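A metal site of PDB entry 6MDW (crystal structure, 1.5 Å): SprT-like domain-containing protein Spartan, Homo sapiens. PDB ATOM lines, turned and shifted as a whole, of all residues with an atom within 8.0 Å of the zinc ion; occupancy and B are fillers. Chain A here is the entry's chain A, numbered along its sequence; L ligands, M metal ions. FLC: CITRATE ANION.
The zinc ion is bound by NE2 of His 91, NE2 of His 110, NE2 of His 95, OHB of the ligand, OB2 of the ligand and OA2 of the ligand.
ND1 of His 110 sits at hydrogen-bond distance from O of Val 131 (3.4 Å). ND1 of His 91 lies within hydrogen-bond range of O of Thr 130 (2.8 Å).
Within 4 Å of the zinc ion: His 91, His 95 and His 110. The nearest printed residue that does not touch the zinc ion is His 133 (4.1 Å).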
ATOM      1  N   GLY A  57      30.494 -17.527  20.119  1.00  0.00           N
ATOM      2  CA  GLY A  57      31.571 -17.906  21.002  1.00  0.00           C
ATOM      3  C   GLY A  57      31.236 -19.213  21.716  1.00  0.00           C
ATOM      4  O   GLY A  57      30.059 -19.451  22.029  1.00  0.00           O
ATOM      5  N   ILE A  58      32.258 -20.030  21.975  1.00  0.00           N
ATOM      6  CA  ILE A  58      32.121 -21.209  22.786  1.00  0.00           C
ATOM      7  C   ILE A  58      33.368 -21.377  23.677  1.00  0.00           C
ATOM      8  O   ILE A  58      34.439 -20.817  23.415  1.00  0.00           O
ATOM      9  CB  ILE A  58      31.880 -22.496  21.949  1.00  0.00           C
ATOM     10  CG1 ILE A  58      33.066 -22.894  21.077  1.00  0.00           C
ATOM     11  CG2 ILE A  58      30.605 -22.357  21.112  1.00  0.00           C
ATOM     12  CD1 ILE A  58      34.128 -23.712  21.783  1.00  0.00           C
ATOM     13  N   CYS A  59      33.221 -22.189  24.718  1.00  0.00           N
ATOM     14  CA  CYS A  59      34.319 -22.804  25.439  1.00  0.00           C
ATOM     15  C   CYS A  59      34.251 -24.331  25.308  1.00  0.00           C
ATOM     16  O   CYS A  59      33.196 -24.918  25.226  1.00  0.00           O
ATOM     17  CB  CYS A  59      34.236 -22.506  26.927  1.00  0.00           C
ATOM     18  SG  CYS A  59      34.433 -20.757  27.342  1.00  0.00           S
ATOM     19  N   TYR A  61      35.995 -27.533  27.726  1.00  0.00           N
ATOM     20  CA  TYR A  61      36.745 -27.816  28.938  1.00  0.00           C
ATOM     21  C   TYR A  61      37.145 -29.286  28.933  1.00  0.00           C
ATOM     22  O   TYR A  61      36.265 -30.136  28.803  1.00  0.00           O
ATOM     23  CB  TYR A  61      35.888 -27.539  30.165  1.00  0.00           C
ATOM     24  CG  TYR A  61      34.907 -26.406  30.021  1.00  0.00           C
ATOM     25  CD1 TYR A  61      33.663 -26.583  29.414  1.00  0.00           C
ATOM     26  CD2 TYR A  61      35.212 -25.157  30.508  1.00  0.00           C
ATOM     27  CE1 TYR A  61      32.759 -25.535  29.311  1.00  0.00           C
ATOM     28  CE2 TYR A  61      34.321 -24.113  30.434  1.00  0.00           C
ATOM     29  CZ  TYR A  61      33.099 -24.289  29.825  1.00  0.00           C
ATOM     30  OH  TYR A  61      32.254 -23.220  29.775  1.00  0.00           O
ATOM     31  N   THR A  88      31.723 -10.669  23.372  1.00  0.00           N
ATOM     32  CA  THR A  88      31.630 -12.121  23.213  1.00  0.00           C
ATOM     33  C   THR A  88      32.848 -12.779  23.900  1.00  0.00           C
ATOM     34  O   THR A  88      32.720 -13.748  24.648  1.00  0.00           O
ATOM     35  CB  THR A  88      31.533 -12.559  21.738  1.00  0.00           C
ATOM     36  OG1 THR A  88      30.368 -11.938  21.176  1.00  0.00           O
ATOM     37  CG2 THR A  88      31.467 -14.063  21.627  1.00  0.00           C
ATOM     38  N   HIS A  91      32.587 -12.594  27.706  1.00  0.00           N
ATOM     39  CA  HIS A  91      31.604 -13.561  28.173  1.00  0.00           C
ATOM     40  C   HIS A  91      32.224 -14.956  28.272  1.00  0.00           C
ATOM     41  O   HIS A  91      32.116 -15.623  29.297  1.00  0.00           O
ATOM     42  CB  HIS A  91      30.391 -13.553  27.229  1.00  0.00           C
ATOM     43  CG  HIS A  91      29.313 -14.521  27.545  1.00  0.00           C
ATOM     44  ND1 HIS A  91      28.028 -14.112  27.886  1.00  0.00           N
ATOM     45  CD2 HIS A  91      29.289 -15.884  27.549  1.00  0.00           C
ATOM     46  CE1 HIS A  91      27.283 -15.196  28.103  1.00  0.00           C
ATOM     47  NE2 HIS A  91      28.033 -16.292  27.913  1.00  0.00           N
ATOM     48  N   GLU A  92      32.901 -15.386  27.208  1.00  0.00           N
ATOM     49  CA  GLU A  92      33.541 -16.686  27.213  1.00  0.00           C
ATOM     50  C   GLU A  92      34.634 -16.776  28.283  1.00  0.00           C
ATOM     51  O   GLU A  92      34.811 -17.796  28.925  1.00  0.00           O
ATOM     52  CB  GLU A  92      34.138 -17.045  25.847  1.00  0.00           C
ATOM     53  CG  GLU A  92      33.119 -17.098  24.719  1.00  0.00           C
ATOM     54  CD  GLU A  92      31.919 -17.961  25.009  1.00  0.00           C
ATOM     55  OE1 GLU A  92      32.014 -18.985  25.711  1.00  0.00           O
ATOM     56  OE2 GLU A  92      30.821 -17.560  24.531  1.00  0.00           O
ATOM     57  N   ILE A  94      34.697 -15.326  31.154  1.00  0.00           N
ATOM     58  CA  ILE A  94      34.068 -15.524  32.449  1.00  0.00           C
ATOM     59  C   ILE A  94      33.772 -17.009  32.647  1.00  0.00           C
ATOM     60  O   ILE A  94      34.083 -17.595  33.672  1.00  0.00           O
ATOM     61  CB  ILE A  94      32.798 -14.684  32.622  1.00  0.00           C
ATOM     62  CG1 ILE A  94      33.132 -13.184  32.591  1.00  0.00           C
ATOM     63  CG2 ILE A  94      32.144 -15.068  33.921  1.00  0.00           C
ATOM     64  CD1 ILE A  94      31.905 -12.333  32.528  1.00  0.00           C
ATOM     65  N   HIS A  95      33.178 -17.653  31.645  1.00  0.00           N
ATOM     66  CA  HIS A  95      32.971 -19.106  31.741  1.00  0.00           C
ATOM     67  C   HIS A  95      34.303 -19.816  31.992  1.00  0.00           C
ATOM     68  O   HIS A  95      34.397 -20.746  32.814  1.00  0.00           O
ATOM     69  CB  HIS A  95      32.343 -19.653  30.451  1.00  0.00           C
ATOM     70  CG  HIS A  95      30.887 -19.344  30.258  1.00  0.00           C
ATOM     71  ND1 HIS A  95      29.902 -19.562  31.212  1.00  0.00           N
ATOM     72  CD2 HIS A  95      30.260 -18.856  29.160  1.00  0.00           C
ATOM     73  CE1 HIS A  95      28.732 -19.188  30.683  1.00  0.00           C
ATOM     74  NE2 HIS A  95      28.928 -18.736  29.428  1.00  0.00           N
ATOM     75  N   GLY A 109      23.237 -21.831  33.591  1.00  0.00           N
ATOM     76  CA  GLY A 109      24.383 -21.568  32.728  1.00  0.00           C
ATOM     77  C   GLY A 109      25.063 -20.267  33.130  1.00  0.00           C
ATOM     78  O   GLY A 109      26.281 -20.192  33.126  1.00  0.00           O
ATOM     79  N   HIS A 110      24.252 -19.245  33.450  1.00  0.00           N
ATOM     80  CA  HIS A 110      24.722 -17.920  33.846  1.00  0.00           C
ATOM     81  C   HIS A 110      24.064 -17.515  35.170  1.00  0.00           C
ATOM     82  O   HIS A 110      23.257 -16.587  35.217  1.00  0.00           O
ATOM     83  CB  HIS A 110      24.404 -16.887  32.778  1.00  0.00           C
ATOM     84  CG  HIS A 110      24.880 -17.324  31.426  1.00  0.00           C
ATOM     85  ND1 HIS A 110      24.085 -18.099  30.600  1.00  0.00           N
ATOM     86  CD2 HIS A 110      26.058 -17.171  30.782  1.00  0.00           C
ATOM     87  CE1 HIS A 110      24.765 -18.391  29.505  1.00  0.00           C
ATOM     88  NE2 HIS A 110      25.963 -17.801  29.580  1.00  0.00           N
ATOM     89  N   PHE A 114      28.329 -15.952  37.512  1.00  0.00           N
ATOM     90  CA  PHE A 114      28.580 -15.362  36.209  1.00  0.00           C
ATOM     91  C   PHE A 114      28.285 -13.860  36.241  1.00  0.00           C
ATOM     92  O   PHE A 114      29.000 -13.025  35.657  1.00  0.00           O
ATOM     93  CB  PHE A 114      27.742 -16.068  35.135  1.00  0.00           C
ATOM     94  CG  PHE A 114      28.142 -15.690  33.736  1.00  0.00           C
ATOM     95  CD1 PHE A 114      27.721 -14.496  33.172  1.00  0.00           C
ATOM     96  CD2 PHE A 114      29.016 -16.490  33.024  1.00  0.00           C
ATOM     97  CE1 PHE A 114      28.122 -14.145  31.893  1.00  0.00           C
ATOM     98  CE2 PHE A 114      29.404 -16.144  31.737  1.00  0.00           C
ATOM     99  CZ  PHE A 114      28.985 -14.950  31.193  1.00  0.00           C
ATOM    100  N   THR A 130      26.569  -9.506  28.434  1.00  0.00           N
ATOM    101  CA  THR A 130      25.227  -9.964  28.808  1.00  0.00           C
ATOM    102  C   THR A 130      25.180 -11.485  28.926  1.00  0.00           C
ATOM    103  O   THR A 130      26.001 -12.180  28.301  1.00  0.00           O
ATOM    104  CB  THR A 130      24.155  -9.563  27.793  1.00  0.00           C
ATOM    105  OG1 THR A 130      24.515 -10.257  26.588  1.00  0.00           O
ATOM    106  CG2 THR A 130      24.042  -8.065  27.603  1.00  0.00           C
ATOM    107  N   VAL A 131      24.174 -11.946  29.663  1.00  0.00           N
ATOM    108  CA  VAL A 131      23.939 -13.352  29.995  1.00  0.00           C
ATOM    109  C   VAL A 131      23.372 -14.106  28.789  1.00  0.00           C
ATOM    110  O   VAL A 131      23.382 -15.341  28.798  1.00  0.00           O
ATOM    111  CB  VAL A 131      23.001 -13.508  31.215  1.00  0.00           C
ATOM    112  CG1 VAL A 131      23.601 -12.918  32.478  1.00  0.00           C
ATOM    113  CG2 VAL A 131      21.626 -12.921  30.960  1.00  0.00           C
ATOM    114  N   TYR A 132      22.835 -13.389  27.789  1.00  0.00           N
ATOM    115  CA  TYR A 132      22.301 -14.047  26.599  1.00  0.00           C
ATOM    116  C   TYR A 132      23.367 -14.057  25.506  1.00  0.00           C
ATOM    117  O   TYR A 132      24.343 -13.296  25.566  1.00  0.00           O
ATOM    118  CB  TYR A 132      20.966 -13.422  26.168  1.00  0.00           C
ATOM    119  CG  TYR A 132      20.979 -11.935  25.973  1.00  0.00           C
ATOM    120  CD1 TYR A 132      20.693 -11.084  27.027  1.00  0.00           C
ATOM    121  CD2 TYR A 132      21.248 -11.371  24.739  1.00  0.00           C
ATOM    122  CE1 TYR A 132      20.702  -9.714  26.864  1.00  0.00           C
ATOM    123  CE2 TYR A 132      21.237  -9.993  24.557  1.00  0.00           C
ATOM    124  CZ  TYR A 132      20.953  -9.164  25.622  1.00  0.00           C
ATOM    125  OH  TYR A 132      20.971  -7.807  25.488  1.00  0.00           O
ATOM    126  N   HIS A 133      23.211 -14.932  24.515  1.00  0.00           N
ATOM    127  CA  HIS A 133      24.302 -15.183  23.592  1.00  0.00           C
ATOM    128  C   HIS A 133      23.912 -14.772  22.175  1.00  0.00           C
ATOM    129  O   HIS A 133      24.508 -15.238  21.202  1.00  0.00           O
ATOM    130  CB  HIS A 133      24.785 -16.630  23.657  1.00  0.00           C
ATOM    131  CG  HIS A 133      26.274 -16.700  23.703  1.00  0.00           C
ATOM    132  ND1 HIS A 133      27.025 -17.310  22.723  1.00  0.00           N
ATOM    133  CD2 HIS A 133      27.160 -16.189  24.601  1.00  0.00           C
ATOM    134  CE1 HIS A 133      28.307 -17.190  23.014  1.00  0.00           C
ATOM    135  NE2 HIS A 133      28.413 -16.524  24.174  1.00  0.00           N
ATOM    136  N   TRP A 146      18.533 -25.761  23.243  1.00  0.00           N
ATOM    137  CA  TRP A 146      19.949 -26.095  23.088  1.00  0.00           C
ATOM    138  C   TRP A 146      20.261 -27.407  23.817  1.00  0.00           C
ATOM    139  O   TRP A 146      19.785 -27.660  24.933  1.00  0.00           O
ATOM    140  CB  TRP A 146      20.845 -24.957  23.597  1.00  0.00           C
ATOM    141  CG  TRP A 146      20.641 -23.657  22.896  1.00  0.00           C
ATOM    142  CD1 TRP A 146      19.669 -23.358  21.991  1.00  0.00           C
ATOM    143  CD2 TRP A 146      21.411 -22.441  23.067  1.00  0.00           C
ATOM    144  NE1 TRP A 146      19.791 -22.062  21.564  1.00  0.00           N
ATOM    145  CE2 TRP A 146      20.845 -21.475  22.200  1.00  0.00           C
ATOM    146  CE3 TRP A 146      22.520 -22.088  23.829  1.00  0.00           C
ATOM    147  CZ2 TRP A 146      21.353 -20.184  22.099  1.00  0.00           C
ATOM    148  CZ3 TRP A 146      23.024 -20.806  23.729  1.00  0.00           C
ATOM    149  CH2 TRP A 146      22.447 -19.868  22.873  1.00  0.00           C
ATOM    150  N   TYR A 162      27.322 -28.621  19.789  1.00  0.00           N
ATOM    151  CA  TYR A 162      26.028 -27.971  19.907  1.00  0.00           C
ATOM    152  C   TYR A 162      24.999 -28.513  18.925  1.00  0.00           C
ATOM    153  O   TYR A 162      25.305 -28.865  17.774  1.00  0.00           O
ATOM    154  CB  TYR A 162      26.197 -26.461  19.743  1.00  0.00           C
ATOM    155  CG  TYR A 162      26.635 -25.790  21.005  1.00  0.00           C
ATOM    156  CD1 TYR A 162      25.745 -25.511  22.035  1.00  0.00           C
ATOM    157  CD2 TYR A 162      27.976 -25.493  21.227  1.00  0.00           C
ATOM    158  CE1 TYR A 162      26.158 -24.899  23.210  1.00  0.00           C
ATOM    159  CE2 TYR A 162      28.412 -24.902  22.399  1.00  0.00           C
ATOM    160  CZ  TYR A 162      27.498 -24.593  23.391  1.00  0.00           C
ATOM    161  OH  TYR A 162      27.920 -24.008  24.555  1.00  0.00           O
ATOM    162  N   MLZ A 164      21.050 -26.688  18.300  1.00  0.00           N
ATOM    163  CA  MLZ A 164      20.159 -25.567  18.608  1.00  0.00           C
ATOM    164  CB  MLZ A 164      20.881 -24.211  18.401  1.00  0.00           C
ATOM    165  CG  MLZ A 164      22.018 -24.107  19.403  1.00  0.00           C
ATOM    166  CD  MLZ A 164      22.630 -22.707  19.501  1.00  0.00           C
ATOM    167  CE  MLZ A 164      23.870 -22.678  20.351  1.00  0.00           C
ATOM    168  NZ  MLZ A 164      24.450 -21.334  20.382  1.00  0.00           N
ATOM    169  CM  MLZ A 164      25.693 -21.309  21.171  1.00  0.00           C
ATOM    170  C   MLZ A 164      18.957 -25.670  17.704  1.00  0.00           C
ATOM    171  O   MLZ A 164      19.092 -25.625  16.509  1.00  0.00           O
ATOM    172  N   LYS A 193      18.821 -24.639  25.879  1.00  0.00           N
ATOM    173  CA  LYS A 193      18.027 -23.438  25.671  1.00  0.00           C
ATOM    174  C   LYS A 193      16.757 -23.809  24.908  1.00  0.00           C
ATOM    175  O   LYS A 193      16.770 -24.745  24.098  1.00  0.00           O
ATOM    176  CB  LYS A 193      18.835 -22.391  24.902  1.00  0.00           C
ATOM    177  CG  LYS A 193      18.606 -20.948  25.350  1.00  0.00           C
ATOM    178  CD  LYS A 193      19.783 -20.019  25.093  1.00  0.00           C
ATOM    179  CE  LYS A 193      19.552 -18.633  25.643  1.00  0.00           C
ATOM    180  NZ  LYS A 193      20.820 -17.883  25.809  1.00  0.00           N
HETATM  181  CAC FLC L   1      28.825 -19.929  25.996  1.00  0.00           C
HETATM  182  CA  FLC L   1      27.686 -20.883  25.917  1.00  0.00           C
HETATM  183  CB  FLC L   1      26.422 -20.387  26.596  1.00  0.00           C
HETATM  184  CBC FLC L   1      25.923 -19.130  25.970  1.00  0.00           C
HETATM  185  CG  FLC L   1      25.366 -21.489  26.458  1.00  0.00           C
HETATM  186  CGC FLC L   1      24.140 -21.259  27.336  1.00  0.00           C
HETATM  187  OA1 FLC L   1      29.938 -20.348  25.535  1.00  0.00           O
HETATM  188  OA2 FLC L   1      28.632 -18.801  26.523  1.00  0.00           O
HETATM  189  OB1 FLC L   1      25.509 -19.293  24.802  1.00  0.00           O
HETATM  190  OB2 FLC L   1      25.965 -17.989  26.580  1.00  0.00           O
HETATM  191  OG1 FLC L   1      23.984 -21.982  28.347  1.00  0.00           O
HETATM  192  OG2 FLC L   1      23.323 -20.359  27.023  1.00  0.00           O
HETATM  193  OHB FLC L   1      26.720 -20.194  27.979  1.00  0.00           O
HETATM  194 ZN    ZN M   1      27.386 -18.204  28.116  1.00  0.00          ZN
